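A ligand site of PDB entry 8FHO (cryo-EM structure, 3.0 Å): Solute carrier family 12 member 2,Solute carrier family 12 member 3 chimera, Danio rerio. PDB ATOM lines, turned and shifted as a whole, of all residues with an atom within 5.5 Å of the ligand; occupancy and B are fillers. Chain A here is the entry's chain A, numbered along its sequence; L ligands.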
ATOM      1  N   LEU A 719     -18.858 -35.462 -31.751  1.00  0.00           N
ATOM      2  CA  LEU A 719     -18.764 -35.059 -30.348  1.00  0.00           C
ATOM      3  C   LEU A 719     -19.977 -34.209 -29.980  1.00  0.00           C
ATOM      4  O   LEU A 719     -19.936 -32.987 -30.036  1.00  0.00           O
ATOM      5  CB  LEU A 719     -17.473 -34.310 -30.092  1.00  0.00           C
ATOM      6  CG  LEU A 719     -16.252 -35.116 -29.691  1.00  0.00           C
ATOM      7  CD1 LEU A 719     -15.826 -35.999 -30.796  1.00  0.00           C
ATOM      8  CD2 LEU A 719     -15.144 -34.154 -29.376  1.00  0.00           C
ATOM      9  N   THR A 720     -21.047 -34.876 -29.565  1.00  0.00           N
ATOM     10  CA  THR A 720     -22.289 -34.203 -29.211  1.00  0.00           C
ATOM     11  C   THR A 720     -22.413 -33.897 -27.734  1.00  0.00           C
ATOM     12  O   THR A 720     -23.200 -33.027 -27.359  1.00  0.00           O
ATOM     13  CB  THR A 720     -23.492 -35.049 -29.616  1.00  0.00           C
ATOM     14  OG1 THR A 720     -23.330 -36.374 -29.125  1.00  0.00           O
ATOM     15  CG2 THR A 720     -23.659 -35.087 -31.102  1.00  0.00           C
ATOM     16  N   GLY A 721     -21.665 -34.571 -26.875  1.00  0.00           N
ATOM     17  CA  GLY A 721     -22.020 -34.614 -25.482  1.00  0.00           C
ATOM     18  C   GLY A 721     -23.311 -35.380 -25.361  1.00  0.00           C
ATOM     19  O   GLY A 721     -23.550 -36.326 -26.126  1.00  0.00           O
ATOM     20  N   PRO A 722     -24.175 -35.011 -24.432  1.00  0.00           N
ATOM     21  CA  PRO A 722     -25.532 -35.558 -24.440  1.00  0.00           C
ATOM     22  C   PRO A 722     -26.220 -35.176 -25.736  1.00  0.00           C
ATOM     23  O   PRO A 722     -26.231 -34.003 -26.116  1.00  0.00           O
ATOM     24  CB  PRO A 722     -26.201 -34.876 -23.237  1.00  0.00           C
ATOM     25  CG  PRO A 722     -25.088 -34.445 -22.379  1.00  0.00           C
ATOM     26  CD  PRO A 722     -23.956 -34.110 -23.293  1.00  0.00           C
ATOM     27  N   ARG A 726     -27.298 -30.568 -27.979  1.00  0.00           N
ATOM     28  CA  ARG A 726     -27.036 -29.883 -29.225  1.00  0.00           C
ATOM     29  C   ARG A 726     -27.443 -30.775 -30.393  1.00  0.00           C
ATOM     30  O   ARG A 726     -26.615 -31.468 -30.982  1.00  0.00           O
ATOM     31  CB  ARG A 726     -25.571 -29.437 -29.312  1.00  0.00           C
ATOM     32  CG  ARG A 726     -24.522 -30.503 -29.148  1.00  0.00           C
ATOM     33  CD  ARG A 726     -23.241 -29.900 -28.632  1.00  0.00           C
ATOM     34  NE  ARG A 726     -23.096 -30.077 -27.193  1.00  0.00           N
ATOM     35  CZ  ARG A 726     -22.226 -29.421 -26.440  1.00  0.00           C
ATOM     36  NH1 ARG A 726     -21.452 -28.470 -26.945  1.00  0.00           N
ATOM     37  NH2 ARG A 726     -22.136 -29.706 -25.148  1.00  0.00           N
ATOM     38  N   LEU A 729     -25.821 -30.807 -34.456  1.00  0.00           N
ATOM     39  CA  LEU A 729     -24.783 -31.717 -34.925  1.00  0.00           C
ATOM     40  C   LEU A 729     -25.381 -33.046 -35.370  1.00  0.00           C
ATOM     41  O   LEU A 729     -24.996 -33.583 -36.407  1.00  0.00           O
ATOM     42  CB  LEU A 729     -23.755 -31.962 -33.806  1.00  0.00           C
ATOM     43  CG  LEU A 729     -22.595 -30.997 -33.655  1.00  0.00           C
ATOM     44  CD1 LEU A 729     -22.000 -31.138 -32.285  1.00  0.00           C
ATOM     45  CD2 LEU A 729     -21.554 -31.272 -34.709  1.00  0.00           C
ATOM     46  N   GLY A 746     -20.195 -39.480 -29.687  1.00  0.00           N
ATOM     47  CA  GLY A 746     -19.349 -39.575 -28.512  1.00  0.00           C
ATOM     48  C   GLY A 746     -19.879 -38.764 -27.341  1.00  0.00           C
ATOM     49  O   GLY A 746     -20.742 -37.905 -27.478  1.00  0.00           O
ATOM     50  N   HIS A 747     -19.330 -39.051 -26.165  1.00  0.00           N
ATOM     51  CA  HIS A 747     -19.690 -38.360 -24.932  1.00  0.00           C
ATOM     52  C   HIS A 747     -18.663 -38.657 -23.860  1.00  0.00           C
ATOM     53  O   HIS A 747     -18.330 -39.825 -23.629  1.00  0.00           O
ATOM     54  CB  HIS A 747     -21.084 -38.761 -24.467  1.00  0.00           C
ATOM     55  CG  HIS A 747     -21.554 -38.054 -23.242  1.00  0.00           C
ATOM     56  ND1 HIS A 747     -22.659 -38.452 -22.528  1.00  0.00           N
ATOM     57  CD2 HIS A 747     -21.083 -36.952 -22.617  1.00  0.00           C
ATOM     58  CE1 HIS A 747     -22.836 -37.636 -21.500  1.00  0.00           C
ATOM     59  NE2 HIS A 747     -21.896 -36.715 -21.539  1.00  0.00           N
ATOM     60  N   VAL A 748     -18.151 -37.638 -23.193  1.00  0.00           N
ATOM     61  CA  VAL A 748     -17.136 -37.796 -22.161  1.00  0.00           C
ATOM     62  C   VAL A 748     -17.717 -37.321 -20.840  1.00  0.00           C
ATOM     63  O   VAL A 748     -18.225 -36.206 -20.747  1.00  0.00           O
ATOM     64  CB  VAL A 748     -15.854 -37.015 -22.501  1.00  0.00           C
ATOM     65  CG1 VAL A 748     -14.826 -37.227 -21.434  1.00  0.00           C
ATOM     66  CG2 VAL A 748     -15.331 -37.461 -23.835  1.00  0.00           C
ATOM     67  N   ILE A 750     -16.903 -36.071 -17.557  1.00  0.00           N
ATOM     68  CA  ILE A 750     -15.724 -35.472 -16.930  1.00  0.00           C
ATOM     69  C   ILE A 750     -15.798 -35.654 -15.417  1.00  0.00           C
ATOM     70  O   ILE A 750     -16.820 -35.357 -14.786  1.00  0.00           O
ATOM     71  CB  ILE A 750     -15.616 -33.987 -17.281  1.00  0.00           C
ATOM     72  CG1 ILE A 750     -15.492 -33.814 -18.791  1.00  0.00           C
ATOM     73  CG2 ILE A 750     -14.415 -33.372 -16.607  1.00  0.00           C
ATOM     74  CD1 ILE A 750     -14.183 -34.252 -19.329  1.00  0.00           C
ATOM     75  N   LEU A 788     -11.491 -33.701 -21.111  1.00  0.00           N
ATOM     76  CA  LEU A 788     -12.187 -34.024 -22.344  1.00  0.00           C
ATOM     77  C   LEU A 788     -11.232 -34.512 -23.429  1.00  0.00           C
ATOM     78  O   LEU A 788     -11.605 -35.373 -24.239  1.00  0.00           O
ATOM     79  CB  LEU A 788     -12.962 -32.792 -22.822  1.00  0.00           C
ATOM     80  CG  LEU A 788     -14.137 -32.952 -23.775  1.00  0.00           C
ATOM     81  CD1 LEU A 788     -15.032 -31.772 -23.565  1.00  0.00           C
ATOM     82  CD2 LEU A 788     -13.686 -32.992 -25.195  1.00  0.00           C
ATOM     83  N   VAL A 810     -16.019 -34.836 -36.302  1.00  0.00           N
ATOM     84  CA  VAL A 810     -16.763 -33.587 -36.407  1.00  0.00           C
ATOM     85  C   VAL A 810     -17.015 -33.070 -34.998  1.00  0.00           C
ATOM     86  O   VAL A 810     -17.415 -33.825 -34.097  1.00  0.00           O
ATOM     87  CB  VAL A 810     -18.069 -33.755 -37.204  1.00  0.00           C
ATOM     88  CG1 VAL A 810     -17.810 -34.477 -38.496  1.00  0.00           C
ATOM     89  CG2 VAL A 810     -19.118 -34.455 -36.422  1.00  0.00           C
ATOM     90  N   VAL A 811     -16.729 -31.787 -34.788  1.00  0.00           N
ATOM     91  CA  VAL A 811     -16.749 -31.181 -33.471  1.00  0.00           C
ATOM     92  C   VAL A 811     -17.342 -29.783 -33.616  1.00  0.00           C
ATOM     93  O   VAL A 811     -17.220 -29.153 -34.669  1.00  0.00           O
ATOM     94  CB  VAL A 811     -15.337 -31.141 -32.862  1.00  0.00           C
ATOM     95  CG1 VAL A 811     -14.426 -30.249 -33.662  1.00  0.00           C
ATOM     96  CG2 VAL A 811     -15.372 -30.684 -31.422  1.00  0.00           C
ATOM     97  N   GLY A 812     -18.004 -29.310 -32.570  1.00  0.00           N
ATOM     98  CA  GLY A 812     -18.569 -27.982 -32.596  1.00  0.00           C
ATOM     99  C   GLY A 812     -17.516 -26.900 -32.524  1.00  0.00           C
ATOM    100  O   GLY A 812     -16.336 -27.165 -32.745  1.00  0.00           O
ATOM    101  N   PHE A 813     -17.922 -25.680 -32.210  1.00  0.00           N
ATOM    102  CA  PHE A 813     -17.014 -24.544 -32.119  1.00  0.00           C
ATOM    103  C   PHE A 813     -17.070 -23.961 -30.720  1.00  0.00           C
ATOM    104  O   PHE A 813     -18.146 -23.816 -30.140  1.00  0.00           O
ATOM    105  CB  PHE A 813     -17.379 -23.493 -33.162  1.00  0.00           C
ATOM    106  CG  PHE A 813     -16.407 -22.356 -33.247  1.00  0.00           C
ATOM    107  CD1 PHE A 813     -15.322 -22.420 -34.091  1.00  0.00           C
ATOM    108  CD2 PHE A 813     -16.592 -21.203 -32.490  1.00  0.00           C
ATOM    109  CE1 PHE A 813     -14.434 -21.366 -34.171  1.00  0.00           C
ATOM    110  CE2 PHE A 813     -15.706 -20.156 -32.562  1.00  0.00           C
ATOM    111  CZ  PHE A 813     -14.631 -20.234 -33.407  1.00  0.00           C
ATOM    112  N   LYS A 814     -15.897 -23.616 -30.184  1.00  0.00           N
ATOM    113  CA  LYS A 814     -15.827 -22.991 -28.859  1.00  0.00           C
ATOM    114  C   LYS A 814     -16.331 -21.561 -28.932  1.00  0.00           C
ATOM    115  O   LYS A 814     -15.554 -20.644 -29.181  1.00  0.00           O
ATOM    116  CB  LYS A 814     -14.389 -23.007 -28.335  1.00  0.00           C
ATOM    117  CG  LYS A 814     -14.060 -24.159 -27.428  1.00  0.00           C
ATOM    118  CD  LYS A 814     -12.834 -23.858 -26.583  1.00  0.00           C
ATOM    119  CE  LYS A 814     -13.173 -22.933 -25.450  1.00  0.00           C
ATOM    120  NZ  LYS A 814     -14.224 -23.521 -24.597  1.00  0.00           N
ATOM    121  N   LYS A 815     -17.618 -21.363 -28.683  1.00  0.00           N
ATOM    122  CA  LYS A 815     -18.185 -20.034 -28.804  1.00  0.00           C
ATOM    123  C   LYS A 815     -17.645 -19.081 -27.745  1.00  0.00           C
ATOM    124  O   LYS A 815     -17.561 -17.873 -27.979  1.00  0.00           O
ATOM    125  CB  LYS A 815     -19.707 -20.111 -28.724  1.00  0.00           C
ATOM    126  CG  LYS A 815     -20.419 -18.782 -28.779  1.00  0.00           C
ATOM    127  CD  LYS A 815     -21.926 -18.957 -28.675  1.00  0.00           C
ATOM    128  CE  LYS A 815     -22.645 -17.629 -28.745  1.00  0.00           C
ATOM    129  NZ  LYS A 815     -24.113 -17.818 -28.633  1.00  0.00           N
ATOM    130  N   ASN A 816     -17.224 -19.610 -26.604  1.00  0.00           N
ATOM    131  CA  ASN A 816     -16.901 -18.822 -25.423  1.00  0.00           C
ATOM    132  C   ASN A 816     -15.400 -18.791 -25.128  1.00  0.00           C
ATOM    133  O   ASN A 816     -14.992 -18.589 -23.991  1.00  0.00           O
ATOM    134  CB  ASN A 816     -17.672 -19.365 -24.217  1.00  0.00           C
ATOM    135  CG  ASN A 816     -17.202 -20.750 -23.801  1.00  0.00           C
ATOM    136  OD1 ASN A 816     -16.165 -20.905 -23.155  1.00  0.00           O
ATOM    137  ND2 ASN A 816     -17.975 -21.758 -24.172  1.00  0.00           N
ATOM    138  N   TYR A 828      -8.628 -27.740 -26.327  1.00  0.00           N
ATOM    139  CA  TYR A 828      -9.495 -27.743 -27.499  1.00  0.00           C
ATOM    140  C   TYR A 828      -8.684 -27.845 -28.782  1.00  0.00           C
ATOM    141  O   TYR A 828      -9.029 -28.613 -29.680  1.00  0.00           O
ATOM    142  CB  TYR A 828     -10.364 -26.495 -27.534  1.00  0.00           C
ATOM    143  CG  TYR A 828     -11.374 -26.527 -28.653  1.00  0.00           C
ATOM    144  CD1 TYR A 828     -12.534 -27.268 -28.524  1.00  0.00           C
ATOM    145  CD2 TYR A 828     -11.167 -25.844 -29.830  1.00  0.00           C
ATOM    146  CE1 TYR A 828     -13.461 -27.316 -29.546  1.00  0.00           C
ATOM    147  CE2 TYR A 828     -12.083 -25.886 -30.858  1.00  0.00           C
ATOM    148  CZ  TYR A 828     -13.227 -26.618 -30.704  1.00  0.00           C
ATOM    149  OH  TYR A 828     -14.145 -26.674 -31.717  1.00  0.00           O
ATOM    150  N   GLY A 850     -25.102 -20.457 -31.642  1.00  0.00           N
ATOM    151  CA  GLY A 850     -24.556 -21.536 -30.858  1.00  0.00           C
ATOM    152  C   GLY A 850     -25.276 -22.855 -31.088  1.00  0.00           C
ATOM    153  O   GLY A 850     -26.341 -22.931 -31.702  1.00  0.00           O
ATOM    154  N   LEU A 851     -24.668 -23.926 -30.581  1.00  0.00           N
ATOM    155  CA  LEU A 851     -25.224 -25.255 -30.708  1.00  0.00           C
ATOM    156  C   LEU A 851     -25.876 -25.760 -29.433  1.00  0.00           C
ATOM    157  O   LEU A 851     -26.885 -26.474 -29.508  1.00  0.00           O
ATOM    158  CB  LEU A 851     -24.144 -26.248 -31.135  1.00  0.00           C
ATOM    159  CG  LEU A 851     -23.619 -26.126 -32.559  1.00  0.00           C
ATOM    160  CD1 LEU A 851     -22.415 -25.232 -32.597  1.00  0.00           C
ATOM    161  CD2 LEU A 851     -23.282 -27.474 -33.108  1.00  0.00           C
ATOM    162  N   ASN A 852     -25.339 -25.396 -28.275  1.00  0.00           N
ATOM    163  CA  ASN A 852     -25.827 -25.912 -27.004  1.00  0.00           C
ATOM    164  C   ASN A 852     -27.176 -25.282 -26.682  1.00  0.00           C
ATOM    165  O   ASN A 852     -27.244 -24.101 -26.323  1.00  0.00           O
ATOM    166  CB  ASN A 852     -24.812 -25.626 -25.902  1.00  0.00           C
ATOM    167  CG  ASN A 852     -25.066 -26.437 -24.645  1.00  0.00           C
ATOM    168  OD1 ASN A 852     -26.046 -27.162 -24.549  1.00  0.00           O
ATOM    169  ND2 ASN A 852     -24.169 -26.306 -23.678  1.00  0.00           N
ATOM    170  N   LYS A 855     -28.490 -24.329 -22.431  1.00  0.00           N
ATOM    171  CA  LYS A 855     -28.404 -23.006 -21.808  1.00  0.00           C
ATOM    172  C   LYS A 855     -29.613 -22.147 -22.160  1.00  0.00           C
ATOM    173  O   LYS A 855     -30.492 -21.911 -21.325  1.00  0.00           O
ATOM    174  CB  LYS A 855     -27.116 -22.317 -22.241  1.00  0.00           C
ATOM    175  CG  LYS A 855     -25.863 -23.142 -22.012  1.00  0.00           C
ATOM    176  CD  LYS A 855     -24.742 -22.754 -22.975  1.00  0.00           C
ATOM    177  CE  LYS A 855     -24.486 -21.256 -22.974  1.00  0.00           C
ATOM    178  NZ  LYS A 855     -23.966 -20.769 -21.669  1.00  0.00           N
HETATM  179  P1  LIG L   1     -21.483 -24.511 -27.856  1.00  0.00           P
HETATM  180  O1  LIG L   1     -21.431 -23.208 -27.108  1.00  0.00           O
HETATM  181  O2  LIG L   1     -22.803 -24.777 -28.526  1.00  0.00           O
HETATM  182  O3  LIG L   1     -20.284 -24.806 -28.720  1.00  0.00           O
HETATM  183  P2  LIG L   1     -20.099 -25.732 -25.750  1.00  0.00           P
HETATM  184  O4  LIG L   1     -20.402 -26.732 -24.670  1.00  0.00           O
HETATM  185  O5  LIG L   1     -19.627 -24.350 -25.390  1.00  0.00           O
HETATM  186  O6  LIG L   1     -21.370 -25.651 -26.724  1.00  0.00           O
HETATM  187  P3  LIG L   1     -17.467 -26.154 -26.069  1.00  0.00           P
HETATM  188  O7  LIG L   1     -17.488 -26.583 -24.629  1.00  0.00           O
HETATM  189  O8  LIG L   1     -17.016 -24.761 -26.406  1.00  0.00           O
HETATM  190  O9  LIG L   1     -18.934 -26.334 -26.664  1.00  0.00           O
HETATM  191  O10 LIG L   1     -16.640 -27.207 -26.935  1.00  0.00           O
HETATM  192  C1  LIG L   1     -16.906 -27.244 -28.332  1.00  0.00           C
HETATM  193  C2  LIG L   1     -17.324 -28.639 -28.760  1.00  0.00           C
HETATM  194  O11 LIG L   1     -16.645 -29.661 -28.034  1.00  0.00           O
HETATM  195  C3  LIG L   1     -18.782 -28.925 -28.488  1.00  0.00           C
HETATM  196  O12 LIG L   1     -19.641 -28.363 -29.468  1.00  0.00           O
HETATM  197  C4  LIG L   1     -18.792 -30.424 -28.551  1.00  0.00           C
HETATM  198  O13 LIG L   1     -18.795 -30.832 -29.900  1.00  0.00           O
HETATM  199  C5  LIG L   1     -17.479 -30.813 -27.922  1.00  0.00           C
HETATM  200  N1  LIG L   1     -17.746 -31.140 -26.522  1.00  0.00           N
HETATM  201  C6  LIG L   1     -17.819 -30.271 -25.507  1.00  0.00           C
HETATM  202  N2  LIG L   1     -18.104 -30.911 -24.348  1.00  0.00           N
HETATM  203  C7  LIG L   1     -18.226 -32.209 -24.619  1.00  0.00           C
HETATM  204  C8  LIG L   1     -18.501 -33.436 -23.856  1.00  0.00           C
HETATM  205  N3  LIG L   1     -18.722 -33.393 -22.523  1.00  0.00           N
HETATM  206  N4  LIG L   1     -18.536 -34.600 -24.531  1.00  0.00           N
HETATM  207  C9  LIG L   1     -18.319 -34.663 -25.842  1.00  0.00           C
HETATM  208  N5  LIG L   1     -18.049 -33.590 -26.580  1.00  0.00           N
HETATM  209  C10 LIG L   1     -17.987 -32.366 -26.049  1.00  0.00           C
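O of Val 810 lies within hydrogen-bond range of N of Leu 719, at 3.2 Å. OH of Tyr 828 sits at hydrogen-bond distance from O of Gly 812 (2.5 Å). The guanidinium group (NE) of Arg 726 is in hydrogen-bond range of the backbone carbonyl oxygen (O) of Thr 720, at 3.0 Å.
O5 of the ligand sits at hydrogen-bond distance from ND2 of Asn 816 (3.3 Å). O8 of the ligand lies within salt-bridge range of NZ of Lys 814, 3.6 Å away. The backbone NH (N) of Gly 812 is in hydrogen-bond range of an oxygen (O13) of the ligand, at 3.2 Å. An oxygen (O13) of the ligand sits at hydrogen-bond distance from the backbone carbonyl oxygen (O) of Leu 719, at 2.4 Å. O2 of the ligand sits at hydrogen-bond distance from N of Asn 852 (2.6 Å). NH1 of Arg 726 is in salt-bridge range of O4 of the ligand (3.0 Å). O of Val 748 sits at hydrogen-bond distance from N3 of the ligand, at 3.4 Å. The backbone carbonyl oxygen (O) of Phe 813 sits close to an oxygen (O3) of the ligand (2.8 Å). N of Val 748 sits at hydrogen-bond distance from N4 of the ligand. The backbone NH (N) of Leu 851 lies within hydrogen-bond range of an oxygen (O2) of the ligand.
Residues that only touch the ligand: Gly 721 (3.5 Å), His 747 (3.95 Å), Leu 788 (3.3 Å), Val 811 (3.7 Å), Lys 815 (3.9 Å) and Tyr 828 (3.7 Å). Hydrophobic or aromatic side chains within 4 Å of the ligand: Leu 719, His 747, Leu 788, Val 811, Tyr 828 and Leu 851. Within 4 Å of the ligand: Leu 719, Gly 721, Arg 726, His 747, Val 748, Leu 788, Val 811, Gly 812, Phe 813, Lys 814, Lys 815, Asn 816, Tyr 828, Leu 851 and Asn 852.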
